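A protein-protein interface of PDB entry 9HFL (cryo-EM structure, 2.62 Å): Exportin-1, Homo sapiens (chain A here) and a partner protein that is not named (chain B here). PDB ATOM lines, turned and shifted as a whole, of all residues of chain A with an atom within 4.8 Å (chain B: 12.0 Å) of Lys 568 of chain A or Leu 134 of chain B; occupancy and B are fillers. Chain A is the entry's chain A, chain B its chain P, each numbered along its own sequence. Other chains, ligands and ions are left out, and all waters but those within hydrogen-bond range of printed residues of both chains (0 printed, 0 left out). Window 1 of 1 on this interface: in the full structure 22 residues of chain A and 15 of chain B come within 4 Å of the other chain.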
ATOM      1  N   LEU A 525      17.313   3.544 -23.903  1.00  0.00           N
ATOM      2  CA  LEU A 525      16.565   3.896 -22.701  1.00  0.00           C
ATOM      3  C   LEU A 525      17.391   4.788 -21.785  1.00  0.00           C
ATOM      4  O   LEU A 525      16.874   5.756 -21.215  1.00  0.00           O
ATOM      5  CB  LEU A 525      16.129   2.629 -21.965  1.00  0.00           C
ATOM      6  CG  LEU A 525      14.956   1.874 -22.590  1.00  0.00           C
ATOM      7  CD1 LEU A 525      14.891   0.454 -22.057  1.00  0.00           C
ATOM      8  CD2 LEU A 525      13.651   2.605 -22.335  1.00  0.00           C
ATOM      9  N   ILE A 544      12.846   4.231 -30.279  1.00  0.00           N
ATOM     10  CA  ILE A 544      12.823   2.926 -29.623  1.00  0.00           C
ATOM     11  C   ILE A 544      11.658   2.093 -30.140  1.00  0.00           C
ATOM     12  O   ILE A 544      11.804   0.895 -30.422  1.00  0.00           O
ATOM     13  CB  ILE A 544      12.753   3.094 -28.093  1.00  0.00           C
ATOM     14  CG1 ILE A 544      14.036   3.731 -27.559  1.00  0.00           C
ATOM     15  CG2 ILE A 544      12.522   1.748 -27.421  1.00  0.00           C
ATOM     16  CD1 ILE A 544      13.872   4.382 -26.202  1.00  0.00           C
ATOM     17  N   PHE A 561       8.700  -8.818 -22.840  1.00  0.00           N
ATOM     18  CA  PHE A 561       9.050  -7.632 -23.614  1.00  0.00           C
ATOM     19  C   PHE A 561       7.916  -7.234 -24.547  1.00  0.00           C
ATOM     20  O   PHE A 561       7.620  -6.045 -24.700  1.00  0.00           O
ATOM     21  CB  PHE A 561      10.332  -7.878 -24.408  1.00  0.00           C
ATOM     22  CG  PHE A 561      11.086  -6.623 -24.734  1.00  0.00           C
ATOM     23  CD1 PHE A 561      10.815  -5.918 -25.893  1.00  0.00           C
ATOM     24  CD2 PHE A 561      12.058  -6.143 -23.877  1.00  0.00           C
ATOM     25  CE1 PHE A 561      11.502  -4.761 -26.191  1.00  0.00           C
ATOM     26  CE2 PHE A 561      12.749  -4.988 -24.171  1.00  0.00           C
ATOM     27  CZ  PHE A 561      12.470  -4.295 -25.329  1.00  0.00           C
ATOM     28  N   THR A 564       5.162  -5.631 -22.468  1.00  0.00           N
ATOM     29  CA  THR A 564       5.588  -4.304 -22.042  1.00  0.00           C
ATOM     30  C   THR A 564       5.523  -3.313 -23.195  1.00  0.00           C
ATOM     31  O   THR A 564       5.091  -2.170 -23.017  1.00  0.00           O
ATOM     32  CB  THR A 564       7.006  -4.367 -21.475  1.00  0.00           C
ATOM     33  OG1 THR A 564       7.127  -5.501 -20.608  1.00  0.00           O
ATOM     34  CG2 THR A 564       7.328  -3.103 -20.700  1.00  0.00           C
ATOM     35  N   VAL A 565       5.943  -3.737 -24.388  1.00  0.00           N
ATOM     36  CA  VAL A 565       5.907  -2.858 -25.552  1.00  0.00           C
ATOM     37  C   VAL A 565       4.470  -2.470 -25.876  1.00  0.00           C
ATOM     38  O   VAL A 565       4.167  -1.302 -26.142  1.00  0.00           O
ATOM     39  CB  VAL A 565       6.593  -3.541 -26.751  1.00  0.00           C
ATOM     40  CG1 VAL A 565       6.187  -2.879 -28.057  1.00  0.00           C
ATOM     41  CG2 VAL A 565       8.101  -3.516 -26.584  1.00  0.00           C
ATOM     42  N   VAL A 566       3.564  -3.449 -25.860  1.00  0.00           N
ATOM     43  CA  VAL A 566       2.170  -3.172 -26.196  1.00  0.00           C
ATOM     44  C   VAL A 566       1.540  -2.245 -25.162  1.00  0.00           C
ATOM     45  O   VAL A 566       0.797  -1.318 -25.509  1.00  0.00           O
ATOM     46  CB  VAL A 566       1.388  -4.490 -26.333  1.00  0.00           C
ATOM     47  CG1 VAL A 566      -0.093  -4.210 -26.484  1.00  0.00           C
ATOM     48  CG2 VAL A 566       1.903  -5.286 -27.518  1.00  0.00           C
ATOM     49  N   ASN A 567       1.812  -2.481 -23.876  1.00  0.00           N
ATOM     50  CA  ASN A 567       1.267  -1.609 -22.842  1.00  0.00           C
ATOM     51  C   ASN A 567       1.844  -0.204 -22.948  1.00  0.00           C
ATOM     52  O   ASN A 567       1.136   0.782 -22.716  1.00  0.00           O
ATOM     53  CB  ASN A 567       1.534  -2.205 -21.462  1.00  0.00           C
ATOM     54  CG  ASN A 567       0.577  -3.331 -21.121  1.00  0.00           C
ATOM     55  OD1 ASN A 567      -0.638  -3.144 -21.105  1.00  0.00           O
ATOM     56  ND2 ASN A 567       1.122  -4.509 -20.846  1.00  0.00           N
ATOM     57  N   LYS A 568       3.126  -0.088 -23.302  1.00  0.00           N
ATOM     58  CA  LYS A 568       3.714   1.227 -23.529  1.00  0.00           C
ATOM     59  C   LYS A 568       3.035   1.934 -24.693  1.00  0.00           C
ATOM     60  O   LYS A 568       2.808   3.146 -24.645  1.00  0.00           O
ATOM     61  CB  LYS A 568       5.214   1.094 -23.794  1.00  0.00           C
ATOM     62  CG  LYS A 568       6.077   0.905 -22.553  1.00  0.00           C
ATOM     63  CD  LYS A 568       5.865   1.991 -21.502  1.00  0.00           C
ATOM     64  CE  LYS A 568       5.874   3.386 -22.102  1.00  0.00           C
ATOM     65  NZ  LYS A 568       5.773   4.428 -21.050  1.00  0.00           N
ATOM     66  N   LEU A 569       2.728   1.196 -25.761  1.00  0.00           N
ATOM     67  CA  LEU A 569       2.017   1.794 -26.886  1.00  0.00           C
ATOM     68  C   LEU A 569       0.635   2.278 -26.466  1.00  0.00           C
ATOM     69  O   LEU A 569       0.204   3.370 -26.856  1.00  0.00           O
ATOM     70  CB  LEU A 569       1.912   0.787 -28.030  1.00  0.00           C
ATOM     71  CG  LEU A 569       3.240   0.433 -28.698  1.00  0.00           C
ATOM     72  CD1 LEU A 569       3.089  -0.770 -29.607  1.00  0.00           C
ATOM     73  CD2 LEU A 569       3.769   1.624 -29.468  1.00  0.00           C
ATOM     74  N   PHE A 570      -0.074   1.481 -25.665  1.00  0.00           N
ATOM     75  CA  PHE A 570      -1.376   1.917 -25.168  1.00  0.00           C
ATOM     76  C   PHE A 570      -1.242   3.171 -24.314  1.00  0.00           C
ATOM     77  O   PHE A 570      -2.087   4.070 -24.380  1.00  0.00           O
ATOM     78  CB  PHE A 570      -2.043   0.796 -24.370  1.00  0.00           C
ATOM     79  CG  PHE A 570      -2.395  -0.417 -25.189  1.00  0.00           C
ATOM     80  CD1 PHE A 570      -2.497  -0.346 -26.569  1.00  0.00           C
ATOM     81  CD2 PHE A 570      -2.623  -1.632 -24.573  1.00  0.00           C
ATOM     82  CE1 PHE A 570      -2.816  -1.460 -27.312  1.00  0.00           C
ATOM     83  CE2 PHE A 570      -2.944  -2.749 -25.312  1.00  0.00           C
ATOM     84  CZ  PHE A 570      -3.040  -2.663 -26.683  1.00  0.00           C
ATOM     85  N   GLU A 571      -0.193   3.242 -23.495  1.00  0.00           N
ATOM     86  CA  GLU A 571       0.047   4.444 -22.700  1.00  0.00           C
ATOM     87  C   GLU A 571       0.322   5.649 -23.592  1.00  0.00           C
ATOM     88  O   GLU A 571      -0.176   6.749 -23.333  1.00  0.00           O
ATOM     89  CB  GLU A 571       1.217   4.207 -21.743  1.00  0.00           C
ATOM     90  CG  GLU A 571       1.436   5.321 -20.731  1.00  0.00           C
ATOM     91  CD  GLU A 571       2.880   5.413 -20.274  1.00  0.00           C
ATOM     92  OE1 GLU A 571       3.255   4.684 -19.333  1.00  0.00           O
ATOM     93  OE2 GLU A 571       3.639   6.214 -20.858  1.00  0.00           O
ATOM     94  N   PHE A 572       1.124   5.460 -24.642  1.00  0.00           N
ATOM     95  CA  PHE A 572       1.417   6.551 -25.566  1.00  0.00           C
ATOM     96  C   PHE A 572       0.167   6.999 -26.309  1.00  0.00           C
ATOM     97  O   PHE A 572       0.061   8.168 -26.696  1.00  0.00           O
ATOM     98  CB  PHE A 572       2.488   6.125 -26.573  1.00  0.00           C
ATOM     99  CG  PHE A 572       3.876   6.031 -25.997  1.00  0.00           C
ATOM    100  CD1 PHE A 572       4.333   6.957 -25.074  1.00  0.00           C
ATOM    101  CD2 PHE A 572       4.730   5.016 -26.395  1.00  0.00           C
ATOM    102  CE1 PHE A 572       5.608   6.865 -24.554  1.00  0.00           C
ATOM    103  CE2 PHE A 572       6.004   4.921 -25.877  1.00  0.00           C
ATOM    104  CZ  PHE A 572       6.444   5.847 -24.956  1.00  0.00           C
ATOM    105  N   GLN B 125      18.079 -12.778 -17.782  1.00  0.00           N
ATOM    106  CA  GLN B 125      17.855 -11.812 -16.712  1.00  0.00           C
ATOM    107  C   GLN B 125      18.124 -10.390 -17.184  1.00  0.00           C
ATOM    108  O   GLN B 125      17.415  -9.457 -16.794  1.00  0.00           O
ATOM    109  CB  GLN B 125      18.728 -12.153 -15.505  1.00  0.00           C
ATOM    110  CG  GLN B 125      18.274 -13.392 -14.756  1.00  0.00           C
ATOM    111  CD  GLN B 125      19.206 -13.765 -13.626  1.00  0.00           C
ATOM    112  OE1 GLN B 125      20.358 -13.340 -13.590  1.00  0.00           O
ATOM    113  NE2 GLN B 125      18.711 -14.570 -12.695  1.00  0.00           N
ATOM    114  N   ASN B 126      19.152 -10.200 -18.014  1.00  0.00           N
ATOM    115  CA  ASN B 126      19.412  -8.880 -18.579  1.00  0.00           C
ATOM    116  C   ASN B 126      18.263  -8.433 -19.469  1.00  0.00           C
ATOM    117  O   ASN B 126      17.870  -7.259 -19.453  1.00  0.00           O
ATOM    118  CB  ASN B 126      20.724  -8.899 -19.363  1.00  0.00           C
ATOM    119  CG  ASN B 126      21.349  -7.525 -19.485  1.00  0.00           C
ATOM    120  OD1 ASN B 126      21.134  -6.654 -18.643  1.00  0.00           O
ATOM    121  ND2 ASN B 126      22.128  -7.323 -20.540  1.00  0.00           N
ATOM    122  N   GLN B 127      17.712  -9.355 -20.261  1.00  0.00           N
ATOM    123  CA  GLN B 127      16.543  -9.028 -21.070  1.00  0.00           C
ATOM    124  C   GLN B 127      15.365  -8.622 -20.193  1.00  0.00           C
ATOM    125  O   GLN B 127      14.657  -7.655 -20.498  1.00  0.00           O
ATOM    126  CB  GLN B 127      16.169 -10.222 -21.946  1.00  0.00           C
ATOM    127  CG  GLN B 127      15.635  -9.842 -23.311  1.00  0.00           C
ATOM    128  CD  GLN B 127      15.449 -11.043 -24.212  1.00  0.00           C
ATOM    129  OE1 GLN B 127      16.107 -12.069 -24.040  1.00  0.00           O
ATOM    130  NE2 GLN B 127      14.552 -10.922 -25.183  1.00  0.00           N
ATOM    131  N   ASP B 128      15.136  -9.354 -19.100  1.00  0.00           N
ATOM    132  CA  ASP B 128      14.051  -9.007 -18.187  1.00  0.00           C
ATOM    133  C   ASP B 128      14.277  -7.636 -17.559  1.00  0.00           C
ATOM    134  O   ASP B 128      13.332  -6.857 -17.393  1.00  0.00           O
ATOM    135  CB  ASP B 128      13.920 -10.069 -17.097  1.00  0.00           C
ATOM    136  CG  ASP B 128      13.461 -11.407 -17.636  1.00  0.00           C
ATOM    137  OD1 ASP B 128      12.954 -11.450 -18.776  1.00  0.00           O
ATOM    138  OD2 ASP B 128      13.606 -12.417 -16.918  1.00  0.00           O
ATOM    139  N   ALA B 129      15.520  -7.334 -17.188  1.00  0.00           N
ATOM    140  CA  ALA B 129      15.824  -6.029 -16.611  1.00  0.00           C
ATOM    141  C   ALA B 129      15.582  -4.915 -17.619  1.00  0.00           C
ATOM    142  O   ALA B 129      15.066  -3.849 -17.267  1.00  0.00           O
ATOM    143  CB  ALA B 129      17.269  -5.999 -16.119  1.00  0.00           C
ATOM    144  N   VAL B 130      15.956  -5.139 -18.880  1.00  0.00           N
ATOM    145  CA  VAL B 130      15.712  -4.134 -19.908  1.00  0.00           C
ATOM    146  C   VAL B 130      14.215  -3.954 -20.129  1.00  0.00           C
ATOM    147  O   VAL B 130      13.737  -2.835 -20.337  1.00  0.00           O
ATOM    148  CB  VAL B 130      16.439  -4.510 -21.211  1.00  0.00           C
ATOM    149  CG1 VAL B 130      15.976  -3.625 -22.356  1.00  0.00           C
ATOM    150  CG2 VAL B 130      17.941  -4.394 -21.026  1.00  0.00           C
ATOM    151  N   ALA B 131      13.453  -5.049 -20.096  1.00  0.00           N
ATOM    152  CA  ALA B 131      12.003  -4.940 -20.219  1.00  0.00           C
ATOM    153  C   ALA B 131      11.416  -4.140 -19.063  1.00  0.00           C
ATOM    154  O   ALA B 131      10.533  -3.298 -19.264  1.00  0.00           O
ATOM    155  CB  ALA B 131      11.376  -6.331 -20.279  1.00  0.00           C
ATOM    156  N   THR B 132      11.897  -4.390 -17.844  1.00  0.00           N
ATOM    157  CA  THR B 132      11.424  -3.634 -16.689  1.00  0.00           C
ATOM    158  C   THR B 132      11.763  -2.156 -16.825  1.00  0.00           C
ATOM    159  O   THR B 132      10.943  -1.290 -16.501  1.00  0.00           O
ATOM    160  CB  THR B 132      12.034  -4.203 -15.408  1.00  0.00           C
ATOM    161  OG1 THR B 132      11.758  -5.607 -15.325  1.00  0.00           O
ATOM    162  CG2 THR B 132      11.462  -3.502 -14.185  1.00  0.00           C
ATOM    163  N   GLU B 133      12.971  -1.849 -17.297  1.00  0.00           N
ATOM    164  CA  GLU B 133      13.349  -0.455 -17.513  1.00  0.00           C
ATOM    165  C   GLU B 133      12.458   0.192 -18.565  1.00  0.00           C
ATOM    166  O   GLU B 133      12.045   1.349 -18.417  1.00  0.00           O
ATOM    167  CB  GLU B 133      14.819  -0.376 -17.925  1.00  0.00           C
ATOM    168  CG  GLU B 133      15.354   1.035 -18.130  1.00  0.00           C
ATOM    169  CD  GLU B 133      14.707   2.055 -17.216  1.00  0.00           C
ATOM    170  OE1 GLU B 133      14.934   1.984 -15.990  1.00  0.00           O
ATOM    171  OE2 GLU B 133      13.976   2.931 -17.723  1.00  0.00           O
ATOM    172  N   LEU B 134      12.154  -0.539 -19.638  1.00  0.00           N
ATOM    173  CA  LEU B 134      11.243  -0.031 -20.655  1.00  0.00           C
ATOM    174  C   LEU B 134       9.852   0.204 -20.087  1.00  0.00           C
ATOM    175  O   LEU B 134       9.148   1.120 -20.525  1.00  0.00           O
ATOM    176  CB  LEU B 134      11.181  -1.010 -21.829  1.00  0.00           C
ATOM    177  CG  LEU B 134      10.161  -0.726 -22.933  1.00  0.00           C
ATOM    178  CD1 LEU B 134      10.450   0.600 -23.617  1.00  0.00           C
ATOM    179  CD2 LEU B 134      10.159  -1.859 -23.942  1.00  0.00           C
ATOM    180  N   GLY B 135       9.436  -0.611 -19.116  1.00  0.00           N
ATOM    181  CA  GLY B 135       8.108  -0.447 -18.548  1.00  0.00           C
ATOM    182  C   GLY B 135       7.907   0.912 -17.905  1.00  0.00           C
ATOM    183  O   GLY B 135       6.840   1.516 -18.031  1.00  0.00           O
ATOM    184  N   ILE B 136       8.929   1.414 -17.215  1.00  0.00           N
ATOM    185  CA  ILE B 136       8.819   2.678 -16.494  1.00  0.00           C
ATOM    186  C   ILE B 136       9.278   3.823 -17.386  1.00  0.00           C
ATOM    187  O   ILE B 136       9.482   4.947 -16.913  1.00  0.00           O
ATOM    188  CB  ILE B 136       9.625   2.652 -15.180  1.00  0.00           C
ATOM    189  CG1 ILE B 136      11.009   2.035 -15.397  1.00  0.00           C
ATOM    190  CG2 ILE B 136       8.865   1.881 -14.112  1.00  0.00           C
ATOM    191  CD1 ILE B 136      11.962   2.257 -14.248  1.00  0.00           C
ATOM    192  N   LEU B 137       9.444   3.552 -18.679  1.00  0.00           N
ATOM    193  CA  LEU B 137       9.787   4.606 -19.624  1.00  0.00           C
ATOM    194  C   LEU B 137       8.694   5.666 -19.635  1.00  0.00           C
ATOM    195  O   LEU B 137       7.502   5.347 -19.622  1.00  0.00           O
ATOM    196  CB  LEU B 137       9.978   4.016 -21.022  1.00  0.00           C
ATOM    197  CG  LEU B 137       9.950   4.971 -22.219  1.00  0.00           C
ATOM    198  CD1 LEU B 137      11.077   5.984 -22.140  1.00  0.00           C
ATOM    199  CD2 LEU B 137      10.034   4.185 -23.516  1.00  0.00           C
ATOM    200  N   GLY B 138       9.103   6.934 -19.653  1.00  0.00           N
ATOM    201  CA  GLY B 138       8.171   8.043 -19.651  1.00  0.00           C
ATOM    202  C   GLY B 138       8.626   9.148 -20.585  1.00  0.00           C
ATOM    203  O   GLY B 138       9.711   9.092 -21.170  1.00  0.00           O
ATOM    204  N   MET B 139       7.762  10.156 -20.712  1.00  0.00           N
ATOM    205  CA  MET B 139       8.063  11.309 -21.550  1.00  0.00           C
ATOM    206  C   MET B 139       7.650  12.622 -20.898  1.00  0.00           C
ATOM    207  O   MET B 139       7.639  13.655 -21.579  1.00  0.00           O
ATOM    208  CB  MET B 139       7.374  11.170 -22.911  1.00  0.00           C
ATOM    209  CG  MET B 139       7.981  10.093 -23.800  1.00  0.00           C
ATOM    210  SD  MET B 139       7.156   9.842 -25.387  1.00  0.00           S
ATOM    211  CE  MET B 139       5.937  11.151 -25.402  1.00  0.00           C
ATOM    212  N   GLU B 140       7.313  12.622 -19.610  1.00  0.00           N
ATOM    213  CA  GLU B 140       6.858  13.818 -18.912  1.00  0.00           C
ATOM    214  C   GLU B 140       7.889  14.359 -17.935  1.00  0.00           C
ATOM    215  O   GLU B 140       8.208  15.551 -17.970  1.00  0.00           O
ATOM    216  CB  GLU B 140       5.547  13.523 -18.167  1.00  0.00           C
ATOM    217  CG  GLU B 140       4.411  13.062 -19.068  1.00  0.00           C
ATOM    218  CD  GLU B 140       3.640  14.220 -19.674  1.00  0.00           C
ATOM    219  OE1 GLU B 140       4.281  15.184 -20.139  1.00  0.00           O
ATOM    220  OE2 GLU B 140       2.393  14.164 -19.687  1.00  0.00           O
ATOM    221  N   GLY B 141       8.424  13.512 -17.058  1.00  0.00           N
ATOM    222  CA  GLY B 141       9.383  13.947 -16.066  1.00  0.00           C
ATOM    223  C   GLY B 141      10.322  12.822 -15.692  1.00  0.00           C
ATOM    224  O   GLY B 141      10.205  11.697 -16.180  1.00  0.00           O
ATOM    225  N   ILE B 143      11.917  10.171 -13.035  1.00  0.00           N
ATOM    226  CA  ILE B 143      11.490   9.357 -11.904  1.00  0.00           C
ATOM    227  C   ILE B 143      12.728   8.922 -11.134  1.00  0.00           C
ATOM    228  O   ILE B 143      13.665   8.361 -11.715  1.00  0.00           O
ATOM    229  CB  ILE B 143      10.666   8.140 -12.364  1.00  0.00           C
ATOM    230  CG1 ILE B 143      10.012   7.456 -11.164  1.00  0.00           C
ATOM    231  CG2 ILE B 143      11.539   7.150 -13.116  1.00  0.00           C
ATOM    232  CD1 ILE B 143       9.162   6.263 -11.536  1.00  0.00           C
ATOM    233  N   ARG B 145      15.283   6.857  -8.948  1.00  0.00           N
ATOM    234  CA  ARG B 145      15.613   5.440  -8.868  1.00  0.00           C
ATOM    235  C   ARG B 145      16.195   5.074  -7.506  1.00  0.00           C
ATOM    236  O   ARG B 145      16.943   4.103  -7.383  1.00  0.00           O
ATOM    237  CB  ARG B 145      16.589   5.053  -9.979  1.00  0.00           C
ATOM    238  CG  ARG B 145      16.218   5.573 -11.362  1.00  0.00           C
ATOM    239  CD  ARG B 145      14.884   5.020 -11.840  1.00  0.00           C
ATOM    240  NE  ARG B 145      14.384   5.734 -13.009  1.00  0.00           N
ATOM    241  CZ  ARG B 145      14.482   5.305 -14.261  1.00  0.00           C
ATOM    242  NH1 ARG B 145      15.075   4.160 -14.560  1.00  0.00           N
ATOM    243  NH2 ARG B 145      13.974   6.046 -15.241  1.00  0.00           N
ATOM    244  N   GLN B 148      15.427   1.439  -6.292  1.00  0.00           N
ATOM    245  CA  GLN B 148      15.876   0.307  -7.094  1.00  0.00           C
ATOM    246  C   GLN B 148      14.709  -0.577  -7.522  1.00  0.00           C
ATOM    247  O   GLN B 148      13.797  -0.109  -8.209  1.00  0.00           O
ATOM    248  CB  GLN B 148      16.920  -0.499  -6.317  1.00  0.00           C
ATOM    249  CG  GLN B 148      18.224   0.247  -6.091  1.00  0.00           C
ATOM    250  CD  GLN B 148      18.308   0.874  -4.714  1.00  0.00           C
ATOM    251  OE1 GLN B 148      17.355   1.489  -4.241  1.00  0.00           O
ATOM    252  NE2 GLN B 148      19.455   0.722  -4.063  1.00  0.00           N
ATOM    253  N   THR B 151      11.078   0.589  -7.307  1.00  0.00           N
ATOM    254  CA  THR B 151      10.670   1.819  -7.969  1.00  0.00           C
ATOM    255  C   THR B 151       9.321   1.637  -8.650  1.00  0.00           C
ATOM    256  O   THR B 151       9.032   0.588  -9.233  1.00  0.00           O
ATOM    257  CB  THR B 151      11.718   2.243  -8.999  1.00  0.00           C
ATOM    258  OG1 THR B 151      13.014   2.267  -8.389  1.00  0.00           O
ATOM    259  CG2 THR B 151      11.398   3.623  -9.551  1.00  0.00           C
ATOM    260  N   TYR B 152       8.488   2.670  -8.567  1.00  0.00           N
ATOM    261  CA  TYR B 152       7.205   2.682  -9.248  1.00  0.00           C
ATOM    262  C   TYR B 152       6.852   4.124  -9.576  1.00  0.00           C
ATOM    263  O   TYR B 152       7.328   5.062  -8.933  1.00  0.00           O
ATOM    264  CB  TYR B 152       6.107   2.028  -8.398  1.00  0.00           C
ATOM    265  CG  TYR B 152       5.728   2.818  -7.168  1.00  0.00           C
ATOM    266  CD1 TYR B 152       6.475   2.728  -6.003  1.00  0.00           C
ATOM    267  CD2 TYR B 152       4.624   3.656  -7.172  1.00  0.00           C
ATOM    268  CE1 TYR B 152       6.132   3.445  -4.879  1.00  0.00           C
ATOM    269  CE2 TYR B 152       4.275   4.380  -6.053  1.00  0.00           C
ATOM    270  CZ  TYR B 152       5.031   4.270  -4.909  1.00  0.00           C
ATOM    271  OH  TYR B 152       4.686   4.991  -3.791  1.00  0.00           O
ATOM    272  N   ASN B 153       6.005   4.292 -10.588  1.00  0.00           N
ATOM    273  CA  ASN B 153       5.630   5.627 -11.031  1.00  0.00           C
ATOM    274  C   ASN B 153       4.710   6.282 -10.011  1.00  0.00           C
ATOM    275  O   ASN B 153       3.492   6.077 -10.037  1.00  0.00           O
ATOM    276  CB  ASN B 153       4.957   5.569 -12.403  1.00  0.00           C
ATOM    277  CG  ASN B 153       5.219   6.809 -13.232  1.00  0.00           C
ATOM    278  OD1 ASN B 153       4.664   7.875 -12.967  1.00  0.00           O
ATOM    279  ND2 ASN B 153       6.071   6.677 -14.242  1.00  0.00           N
ATOM    280  N   LEU B 156       2.753   9.660 -11.686  1.00  0.00           N
ATOM    281  CA  LEU B 156       1.517   9.305 -12.372  1.00  0.00           C
ATOM    282  C   LEU B 156       0.433   8.929 -11.373  1.00  0.00           C
ATOM    283  O   LEU B 156      -0.746   9.237 -11.575  1.00  0.00           O
ATOM    284  CB  LEU B 156       1.772   8.158 -13.349  1.00  0.00           C
ATOM    285  CG  LEU B 156       0.548   7.601 -14.082  1.00  0.00           C
ATOM    286  CD1 LEU B 156      -0.113   8.677 -14.929  1.00  0.00           C
ATOM    287  CD2 LEU B 156       0.942   6.411 -14.941  1.00  0.00           C
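NZ of Lys 568 of chain A is in hydrogen-bond range of O of Leu 137 of chain B, 2.4 Å away.
The side-chain amino group of Lys 568 of chain A is in salt-bridge range of the side-chain carboxylate of Glu 571 of chain A, 2.8 Å away.
The side-chain carboxylate of Glu 133 of chain B lies within salt-bridge range of the guanidinium group of Arg 145 of chain B.
Leu 525 of chain A touches Val 130 of chain B.
Leu 525 of chain A touches Glu 133 of chain B (CD1 to CG, 3.997 Å).
Leu 134 of chain B touches Leu 525 of chain A (N to CD1, 3.8 Å).
Phe 561 of chain A touches Val 130 of chain B (CE2 to CG1, 3.9 Å).
CD2 of Leu 134 of chain B touches CZ of Phe 561 of chain A (3.6 Å).
Thr 564 of chain A touches Ala 131 of chain B.
Thr 564 of chain A touches Gly 135 of chain B.
Lys 568 of chain A touches Leu 134 of chain B (CD to O, 3.5 Å).
Gly 135 of chain B touches Lys 568 of chain A (O to CD, 3.6 Å).
CE1 of Phe 572 of chain A touches SD of Met 139 of chain B, at 3.5 Å.
Lys 568 of chain A touches three residues of chain B.
Leu 134 of chain B touches just these residues of chain A: Leu 525 (3.8 Å), Phe 561 (3.6 Å), Val 565 (3.7 Å) and Lys 568 (3.5 Å).
Phe 561 of chain A touches just these residues of chain B: Val 130 (3.9 Å), Ala 131 (3.7 Å) and Leu 134 (3.6 Å).
Thr 564 of chain A touches just these residues of chain B: Ala 131 and Gly 135.
Of chain B, only Leu 134 (3.7 Å) comes within 4 Å of Val 565 of chain A.
No residue of chain B comes within 4 Å of Val 566 of chain A.
No residue of chain B comes within 4 Å of Glu 571 of chain A.
Of the printed residues of chain B, Phe 572 of chain A touches Met 139 (3.5 Å).
Of the printed residues of chain A, Gly 135 of chain B touches Thr 564 and Lys 568.
Of the printed residues of chain A, Val 130 of chain B touches Leu 525 (3.9 Å) and Phe 561 (3.9 Å).
Asp 128 of chain B touches none of the printed residues of chain A.
Arg 145 of chain B touches none of the printed residues of chain A.
The nearest residue of chain B that does not touch Lys 568 of chain A is Gly 138 of chain B (4.4 Å).
Printed residues of chain A that touch a printed residue of chain B: Leu 525, Phe 561, Thr 564, Val 565, Lys 568 and Phe 572.
Along chain A the printed residues that touch a printed residue of chain B span positions 525 to 572.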
